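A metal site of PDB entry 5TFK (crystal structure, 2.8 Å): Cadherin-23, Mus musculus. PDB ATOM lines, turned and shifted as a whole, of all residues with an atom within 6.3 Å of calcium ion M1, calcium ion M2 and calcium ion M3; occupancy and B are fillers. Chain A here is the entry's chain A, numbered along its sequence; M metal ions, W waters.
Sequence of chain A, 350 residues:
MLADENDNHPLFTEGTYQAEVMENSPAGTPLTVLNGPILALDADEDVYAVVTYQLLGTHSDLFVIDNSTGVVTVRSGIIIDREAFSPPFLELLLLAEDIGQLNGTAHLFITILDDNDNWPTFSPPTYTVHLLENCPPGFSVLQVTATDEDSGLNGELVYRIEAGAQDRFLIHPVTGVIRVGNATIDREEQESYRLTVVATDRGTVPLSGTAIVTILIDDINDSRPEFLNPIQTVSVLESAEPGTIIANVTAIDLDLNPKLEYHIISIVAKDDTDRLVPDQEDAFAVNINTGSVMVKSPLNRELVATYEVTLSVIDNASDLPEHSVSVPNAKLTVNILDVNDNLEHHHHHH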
ATOM      1  N   GLU A  23       6.032  -7.166 -10.668  1.00  0.00           N
ATOM      2  CA  GLU A  23       6.332  -8.580 -10.354  1.00  0.00           C
ATOM      3  C   GLU A  23       7.654  -8.819  -9.594  1.00  0.00           C
ATOM      4  O   GLU A  23       8.584  -8.009  -9.666  1.00  0.00           O
ATOM      5  CB  GLU A  23       6.309  -9.471 -11.628  1.00  0.00           C
ATOM      6  CG  GLU A  23       7.460  -9.228 -12.617  1.00  0.00           C
ATOM      7  CD  GLU A  23       7.665 -10.337 -13.661  1.00  0.00           C
ATOM      8  OE1 GLU A  23       8.415 -10.105 -14.642  1.00  0.00           O
ATOM      9  OE2 GLU A  23       7.093 -11.439 -13.510  1.00  0.00           O
ATOM     10  N   ASN A  24       7.726  -9.942  -8.858  1.00  0.00           N
ATOM     11  CA  ASN A  24       8.873 -10.237  -7.976  1.00  0.00           C
ATOM     12  C   ASN A  24       9.105  -9.150  -6.930  1.00  0.00           C
ATOM     13  O   ASN A  24      10.242  -8.945  -6.492  1.00  0.00           O
ATOM     14  CB  ASN A  24      10.190 -10.429  -8.761  1.00  0.00           C
ATOM     15  CG  ASN A  24      10.078 -11.444  -9.879  1.00  0.00           C
ATOM     16  OD1 ASN A  24       9.626 -12.574  -9.652  1.00  0.00           O
ATOM     17  ND2 ASN A  24      10.483 -11.049 -11.077  1.00  0.00           N
ATOM     18  N   ILE A  80       5.120 -13.413  -6.980  1.00  0.00           N
ATOM     19  CA  ILE A  80       4.250 -13.025  -8.081  1.00  0.00           C
ATOM     20  C   ILE A  80       5.038 -12.966  -9.387  1.00  0.00           C
ATOM     21  O   ILE A  80       6.081 -12.257  -9.433  1.00  0.00           O
ATOM     22  CB  ILE A  80       3.611 -11.658  -7.833  1.00  0.00           C
ATOM     23  CG1 ILE A  80       2.846 -11.676  -6.504  1.00  0.00           C
ATOM     24  CG2 ILE A  80       2.687 -11.281  -8.996  1.00  0.00           C
ATOM     25  CD1 ILE A  80       2.244 -10.355  -6.104  1.00  0.00           C
ATOM     26  N   ASP A  81       4.546 -13.696 -10.392  1.00  0.00           N
ATOM     27  CA  ASP A  81       5.270 -13.923 -11.643  1.00  0.00           C
ATOM     28  C   ASP A  81       4.396 -13.574 -12.828  1.00  0.00           C
ATOM     29  O   ASP A  81       3.353 -14.171 -12.964  1.00  0.00           O
ATOM     30  CB  ASP A  81       5.621 -15.406 -11.725  1.00  0.00           C
ATOM     31  CG  ASP A  81       6.105 -15.812 -13.086  1.00  0.00           C
ATOM     32  OD1 ASP A  81       6.659 -14.954 -13.806  1.00  0.00           O
ATOM     33  OD2 ASP A  81       5.978 -16.997 -13.420  1.00  0.00           O
ATOM     34  N   ARG A  82       4.808 -12.613 -13.663  1.00  0.00           N
ATOM     35  CA  ARG A  82       3.919 -12.073 -14.681  1.00  0.00           C
ATOM     36  C   ARG A  82       3.743 -13.077 -15.816  1.00  0.00           C
ATOM     37  O   ARG A  82       2.746 -13.054 -16.554  1.00  0.00           O
ATOM     38  CB  ARG A  82       4.503 -10.754 -15.193  1.00  0.00           C
ATOM     39  CG  ARG A  82       3.501  -9.885 -15.932  1.00  0.00           C
ATOM     40  CD  ARG A  82       4.189  -8.823 -16.783  1.00  0.00           C
ATOM     41  NE  ARG A  82       5.128  -9.449 -17.703  1.00  0.00           N
ATOM     42  CZ  ARG A  82       4.782 -10.140 -18.788  1.00  0.00           C
ATOM     43  NH1 ARG A  82       3.503 -10.299 -19.142  1.00  0.00           N
ATOM     44  NH2 ARG A  82       5.734 -10.681 -19.543  1.00  0.00           N
ATOM     45  N   GLU A  83       4.722 -13.969 -15.948  1.00  0.00           N
ATOM     46  CA  GLU A  83       4.763 -15.003 -16.976  1.00  0.00           C
ATOM     47  C   GLU A  83       3.789 -16.128 -16.637  1.00  0.00           C
ATOM     48  O   GLU A  83       3.591 -17.021 -17.452  1.00  0.00           O
ATOM     49  CB  GLU A  83       6.174 -15.598 -17.089  1.00  0.00           C
ATOM     50  CG  GLU A  83       7.238 -14.709 -17.732  1.00  0.00           C
ATOM     51  CD  GLU A  83       7.448 -13.376 -17.022  1.00  0.00           C
ATOM     52  OE1 GLU A  83       8.119 -13.317 -15.971  1.00  0.00           O
ATOM     53  OE2 GLU A  83       6.929 -12.376 -17.549  1.00  0.00           O
ATOM     54  N   ALA A  84       3.225 -16.117 -15.424  1.00  0.00           N
ATOM     55  CA  ALA A  84       2.236 -17.122 -15.018  1.00  0.00           C
ATOM     56  C   ALA A  84       0.790 -16.605 -15.091  1.00  0.00           C
ATOM     57  O   ALA A  84      -0.138 -17.338 -14.751  1.00  0.00           O
ATOM     58  CB  ALA A  84       2.561 -17.612 -13.619  1.00  0.00           C
ATOM     59  N   LEU A 113       3.154  -5.489 -13.519  1.00  0.00           N
ATOM     60  CA  LEU A 113       4.056  -4.896 -14.463  1.00  0.00           C
ATOM     61  C   LEU A 113       5.209  -5.849 -14.700  1.00  0.00           C
ATOM     62  O   LEU A 113       5.447  -6.777 -13.913  1.00  0.00           O
ATOM     63  CB  LEU A 113       4.543  -3.533 -13.977  1.00  0.00           C
ATOM     64  CG  LEU A 113       3.471  -2.435 -13.996  1.00  0.00           C
ATOM     65  CD1 LEU A 113       3.687  -1.496 -12.832  1.00  0.00           C
ATOM     66  CD2 LEU A 113       3.444  -1.669 -15.327  1.00  0.00           C
ATOM     67  N   ASP A 114       5.962  -5.598 -15.765  1.00  0.00           N
ATOM     68  CA  ASP A 114       6.966  -6.534 -16.274  1.00  0.00           C
ATOM     69  C   ASP A 114       8.349  -6.193 -15.770  1.00  0.00           C
ATOM     70  O   ASP A 114       8.793  -5.053 -15.871  1.00  0.00           O
ATOM     71  CB  ASP A 114       6.987  -6.532 -17.792  1.00  0.00           C
ATOM     72  CG  ASP A 114       7.815  -7.677 -18.372  1.00  0.00           C
ATOM     73  OD1 ASP A 114       7.774  -8.794 -17.801  1.00  0.00           O
ATOM     74  OD2 ASP A 114       8.505  -7.453 -19.385  1.00  0.00           O
ATOM     75  N   ASP A 115       9.001  -7.207 -15.210  1.00  0.00           N
ATOM     76  CA  ASP A 115      10.391  -7.161 -14.793  1.00  0.00           C
ATOM     77  C   ASP A 115      11.209  -8.013 -15.772  1.00  0.00           C
ATOM     78  O   ASP A 115      10.773  -9.090 -16.161  1.00  0.00           O
ATOM     79  CB  ASP A 115      10.496  -7.738 -13.378  1.00  0.00           C
ATOM     80  CG  ASP A 115      11.908  -7.751 -12.837  1.00  0.00           C
ATOM     81  OD1 ASP A 115      12.736  -6.898 -13.234  1.00  0.00           O
ATOM     82  OD2 ASP A 115      12.162  -8.629 -11.985  1.00  0.00           O
ATOM     83  N   ASN A 116      12.371  -7.537 -16.165  1.00  0.00           N
ATOM     84  CA  ASN A 116      13.163  -8.226 -17.150  1.00  0.00           C
ATOM     85  C   ASN A 116      13.837  -9.417 -16.487  1.00  0.00           C
ATOM     86  O   ASN A 116      15.023  -9.353 -16.188  1.00  0.00           O
ATOM     87  CB  ASN A 116      14.196  -7.281 -17.756  1.00  0.00           C
ATOM     88  CG  ASN A 116      14.839  -7.847 -18.994  1.00  0.00           C
ATOM     89  OD1 ASN A 116      14.246  -8.658 -19.701  1.00  0.00           O
ATOM     90  ND2 ASN A 116      16.082  -7.432 -19.264  1.00  0.00           N
ATOM     91  N   ASP A 117      13.061 -10.476 -16.271  1.00  0.00           N
ATOM     92  CA  ASP A 117      13.492 -11.642 -15.449  1.00  0.00           C
ATOM     93  C   ASP A 117      13.717 -12.940 -16.211  1.00  0.00           C
ATOM     94  O   ASP A 117      13.946 -13.986 -15.607  1.00  0.00           O
ATOM     95  CB  ASP A 117      12.547 -11.900 -14.261  1.00  0.00           C
ATOM     96  CG  ASP A 117      11.123 -12.289 -14.659  1.00  0.00           C
ATOM     97  OD1 ASP A 117      10.638 -11.937 -15.750  1.00  0.00           O
ATOM     98  OD2 ASP A 117      10.436 -12.906 -13.809  1.00  0.00           O
ATOM     99  N   ASN A 118      13.657 -12.858 -17.539  1.00  0.00           N
ATOM    100  CA  ASN A 118      13.817 -14.017 -18.415  1.00  0.00           C
ATOM    101  C   ASN A 118      14.908 -13.729 -19.458  1.00  0.00           C
ATOM    102  O   ASN A 118      14.885 -12.685 -20.112  1.00  0.00           O
ATOM    103  CB  ASN A 118      12.501 -14.328 -19.140  1.00  0.00           C
ATOM    104  CG  ASN A 118      11.514 -15.090 -18.274  1.00  0.00           C
ATOM    105  OD1 ASN A 118      11.355 -16.281 -18.433  1.00  0.00           O
ATOM    106  ND2 ASN A 118      10.801 -14.379 -17.398  1.00  0.00           N
ATOM    107  N   TRP A 119      15.810 -14.695 -19.628  1.00  0.00           N
ATOM    108  CA  TRP A 119      16.941 -14.618 -20.522  1.00  0.00           C
ATOM    109  C   TRP A 119      16.499 -15.012 -21.938  1.00  0.00           C
ATOM    110  O   TRP A 119      15.829 -16.042 -22.160  1.00  0.00           O
ATOM    111  CB  TRP A 119      18.050 -15.586 -20.123  1.00  0.00           C
ATOM    112  CG  TRP A 119      18.904 -15.148 -18.994  1.00  0.00           C
ATOM    113  CD1 TRP A 119      20.143 -14.602 -19.072  1.00  0.00           C
ATOM    114  CD2 TRP A 119      18.604 -15.273 -17.603  1.00  0.00           C
ATOM    115  NE1 TRP A 119      20.631 -14.367 -17.817  1.00  0.00           N
ATOM    116  CE2 TRP A 119      19.701 -14.765 -16.900  1.00  0.00           C
ATOM    117  CE3 TRP A 119      17.508 -15.758 -16.896  1.00  0.00           C
ATOM    118  CZ2 TRP A 119      19.741 -14.736 -15.503  1.00  0.00           C
ATOM    119  CZ3 TRP A 119      17.544 -15.742 -15.509  1.00  0.00           C
ATOM    120  CH2 TRP A 119      18.658 -15.229 -14.829  1.00  0.00           C
ATOM    121  N   PRO A 120      16.904 -14.224 -22.927  1.00  0.00           N
ATOM    122  CA  PRO A 120      16.889 -14.738 -24.319  1.00  0.00           C
ATOM    123  C   PRO A 120      17.537 -16.127 -24.359  1.00  0.00           C
ATOM    124  O   PRO A 120      18.652 -16.306 -23.854  1.00  0.00           O
ATOM    125  CB  PRO A 120      17.732 -13.710 -25.082  1.00  0.00           C
ATOM    126  CG  PRO A 120      17.574 -12.451 -24.306  1.00  0.00           C
ATOM    127  CD  PRO A 120      17.476 -12.859 -22.854  1.00  0.00           C
ATOM    128  N   ASP A 148      12.316 -15.114 -25.578  1.00  0.00           N
ATOM    129  CA  ASP A 148      12.294 -14.463 -24.258  1.00  0.00           C
ATOM    130  C   ASP A 148      10.847 -14.343 -23.753  1.00  0.00           C
ATOM    131  O   ASP A 148       9.995 -13.800 -24.472  1.00  0.00           O
ATOM    132  CB  ASP A 148      12.940 -13.071 -24.435  1.00  0.00           C
ATOM    133  CG  ASP A 148      13.249 -12.360 -23.110  1.00  0.00           C
ATOM    134  OD1 ASP A 148      12.433 -12.423 -22.157  1.00  0.00           O
ATOM    135  OD2 ASP A 148      14.287 -11.669 -23.035  1.00  0.00           O
ATOM    136  N   GLU A 149      10.575 -14.922 -22.585  1.00  0.00           N
ATOM    137  CA  GLU A 149       9.227 -15.002 -22.076  1.00  0.00           C
ATOM    138  C   GLU A 149       8.739 -13.644 -21.605  1.00  0.00           C
ATOM    139  O   GLU A 149       7.560 -13.492 -21.402  1.00  0.00           O
ATOM    140  CB  GLU A 149       9.082 -16.008 -20.940  1.00  0.00           C
ATOM    141  CG  GLU A 149       9.521 -17.425 -21.277  1.00  0.00           C
ATOM    142  CD  GLU A 149       9.002 -17.917 -22.615  1.00  0.00           C
ATOM    143  OE1 GLU A 149       7.861 -18.434 -22.670  1.00  0.00           O
ATOM    144  OE2 GLU A 149       9.748 -17.811 -23.615  1.00  0.00           O
ATOM    145  N   ASP A 150       9.614 -12.663 -21.461  1.00  0.00           N
ATOM    146  CA  ASP A 150       9.181 -11.310 -21.120  1.00  0.00           C
ATOM    147  C   ASP A 150       8.509 -10.625 -22.315  1.00  0.00           C
ATOM    148  O   ASP A 150       8.328 -11.222 -23.391  1.00  0.00           O
ATOM    149  CB  ASP A 150      10.357 -10.491 -20.587  1.00  0.00           C
ATOM    150  CG  ASP A 150      11.026 -11.149 -19.389  1.00  0.00           C
ATOM    151  OD1 ASP A 150      10.292 -11.744 -18.567  1.00  0.00           O
ATOM    152  OD2 ASP A 150      12.278 -11.066 -19.274  1.00  0.00           O
ATOM    153  N   SER A 151       8.064  -9.384 -22.107  1.00  0.00           N
ATOM    154  CA  SER A 151       7.270  -8.679 -23.113  1.00  0.00           C
ATOM    155  C   SER A 151       7.391  -7.174 -22.976  1.00  0.00           C
ATOM    156  O   SER A 151       7.683  -6.651 -21.906  1.00  0.00           O
ATOM    157  CB  SER A 151       5.797  -9.108 -23.064  1.00  0.00           C
ATOM    158  OG  SER A 151       5.254  -8.920 -21.766  1.00  0.00           O
ATOM    159  N   LEU A 153       9.846  -4.232 -24.405  1.00  0.00           N
ATOM    160  CA  LEU A 153      11.273  -4.165 -24.727  1.00  0.00           C
ATOM    161  C   LEU A 153      12.066  -5.280 -24.015  1.00  0.00           C
ATOM    162  O   LEU A 153      13.140  -5.664 -24.478  1.00  0.00           O
ATOM    163  CB  LEU A 153      11.841  -2.793 -24.352  1.00  0.00           C
ATOM    164  CG  LEU A 153      11.252  -1.559 -25.055  1.00  0.00           C
ATOM    165  CD1 LEU A 153      11.735  -0.255 -24.417  1.00  0.00           C
ATOM    166  CD2 LEU A 153      11.553  -1.584 -26.554  1.00  0.00           C
ATOM    167  N   ASN A 154      11.505  -5.810 -22.930  1.00  0.00           N
ATOM    168  CA  ASN A 154      12.106  -6.931 -22.202  1.00  0.00           C
ATOM    169  C   ASN A 154      12.123  -8.248 -22.974  1.00  0.00           C
ATOM    170  O   ASN A 154      12.852  -9.155 -22.611  1.00  0.00           O
ATOM    171  CB  ASN A 154      11.349  -7.160 -20.894  1.00  0.00           C
ATOM    172  CG  ASN A 154      11.427  -5.973 -19.955  1.00  0.00           C
ATOM    173  OD1 ASN A 154      12.224  -5.030 -20.146  1.00  0.00           O
ATOM    174  ND2 ASN A 154      10.599  -6.012 -18.920  1.00  0.00           N
ATOM    175  N   GLY A 155      11.258  -8.367 -23.988  1.00  0.00           N
ATOM    176  CA  GLY A 155      11.194  -9.567 -24.829  1.00  0.00           C
ATOM    177  C   GLY A 155      11.692  -9.424 -26.263  1.00  0.00           C
ATOM    178  O   GLY A 155      11.805 -10.410 -26.975  1.00  0.00           O
ATOM    179  N   LEU A 157      14.292  -8.700 -29.262  1.00  0.00           N
ATOM    180  CA  LEU A 157      15.618  -9.337 -29.336  1.00  0.00           C
ATOM    181  C   LEU A 157      16.429  -8.827 -30.513  1.00  0.00           C
ATOM    182  O   LEU A 157      15.949  -8.836 -31.636  1.00  0.00           O
ATOM    183  CB  LEU A 157      15.476 -10.858 -29.484  1.00  0.00           C
ATOM    184  CG  LEU A 157      14.772 -11.635 -28.373  1.00  0.00           C
ATOM    185  CD1 LEU A 157      14.956 -13.133 -28.563  1.00  0.00           C
ATOM    186  CD2 LEU A 157      15.294 -11.188 -27.016  1.00  0.00           C
ATOM    187  N   ASP A 201      18.048  -8.978 -25.257  1.00  0.00           N
ATOM    188  CA  ASP A 201      16.886  -8.106 -25.057  1.00  0.00           C
ATOM    189  C   ASP A 201      17.189  -6.620 -24.812  1.00  0.00           C
ATOM    190  O   ASP A 201      18.343  -6.190 -24.630  1.00  0.00           O
ATOM    191  CB  ASP A 201      15.917  -8.674 -23.984  1.00  0.00           C
ATOM    192  CG  ASP A 201      16.480  -8.655 -22.568  1.00  0.00           C
ATOM    193  OD1 ASP A 201      17.313  -7.795 -22.204  1.00  0.00           O
ATOM    194  OD2 ASP A 201      16.048  -9.500 -21.758  1.00  0.00           O
ATOM    195  N   GLY A 203      15.601  -4.706 -22.223  1.00  0.00           N
ATOM    196  CA  GLY A 203      15.282  -4.270 -20.860  1.00  0.00           C
ATOM    197  C   GLY A 203      16.396  -3.390 -20.341  1.00  0.00           C
ATOM    198  O   GLY A 203      17.538  -3.486 -20.813  1.00  0.00           O
ATOM    199  N   LEU A 207      19.507  -8.383 -20.662  1.00  0.00           N
ATOM    200  CA  LEU A 207      19.905  -9.795 -20.555  1.00  0.00           C
ATOM    201  C   LEU A 207      20.186 -10.457 -21.923  1.00  0.00           C
ATOM    202  O   LEU A 207      19.566 -10.128 -22.941  1.00  0.00           O
ATOM    203  CB  LEU A 207      18.832 -10.624 -19.830  1.00  0.00           C
ATOM    204  CG  LEU A 207      18.651 -10.462 -18.315  1.00  0.00           C
ATOM    205  CD1 LEU A 207      17.395 -11.172 -17.844  1.00  0.00           C
ATOM    206  CD2 LEU A 207      19.848 -10.992 -17.556  1.00  0.00           C
HETATM  207 CA    CA M   1       8.500 -13.599 -13.565  1.00  0.00          CA
HETATM  208 CA    CA M   2       9.046 -10.597 -16.774  1.00  0.00          CA
HETATM  209 CA    CA M   3      14.148 -10.561 -20.922  1.00  0.00          CA
HETATM  210  O   HOH W   1       9.476 -15.405 -14.640  1.00  0.00           O
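The guanidinium group (NH2) of Arg 82 sits close to the side-chain carboxylate (OE2) of Glu 83. OD2 of Asp 114 is in hydrogen-bond range of ND2 of Asn 154, at 2.6 Å. The side-chain amide nitrogen (ND2) of Asn 24 is in hydrogen-bond range of the side-chain carboxylate (OD2) of Asp 115 (3.1 Å). The side-chain carboxylate (OD2) of Asp 117 lies close to the side-chain amide nitrogen (ND2) of Asn 24 (3.3 Å). The backbone NH (N) of Arg 82 sits close to the side-chain carboxylate (OE2) of Glu 23 (2.6 Å). N of Glu 23 is in hydrogen-bond range of O of Leu 113 (3.3 Å). The guanidinium group (NH2) of Arg 82 is in hydrogen-bond range of the side-chain hydroxyl (OG) of Ser 151, at 2.9 Å. OD2 of Asp 114 lies within hydrogen-bond range of N of Ser 151 (3.4 Å).
Arg 82 touches calcium ion M1 (N to CA, 3.8 Å). Within 4 Å of calcium ion M1: Glu 23, Asp 81, Arg 82, Glu 83 and Asp 117.
Within 4 Å of calcium ion M2: Glu 23, Glu 83, Asp 114, Asp 115, Asp 117 and Asp 150. Along chain A the residues within 4 Å of calcium ion M2 span positions 23 to 150.
Of the 26 residues printed, 6 come within 4 Å of calcium ion M3.
OD2 of Asp 117 is bound to calcium ion M1 (2.1 Å). OD1 of Asp 81 binds calcium ion M1 (2.3 Å). Water W1 binds calcium ion M1. OE1 of Glu 83 binds calcium ion M1, 2.5 Å away. Calcium ion M1 is bound by OE2 of Glu 23. Calcium ion M1 has five donor atoms within binding distance.
Calcium ion M2 is bound by OE1 of Glu 23, OD1 of Asp 117, O of Asp 115, OD1 of Asp 114, OD1 of Asp 150 and OE2 of Glu 83. Slightly farther from calcium ion M2 lies the side-chain carboxylate (OE1) of Glu 83 (3.0 Å).
Calcium ion M3 is bound by OD1 of Asn 116, OD2 of Asp 201, OD2 of Asp 148, O of Asn 118, OD2 of Asp 150, O of Asn 154 and OD1 of Asp 148.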
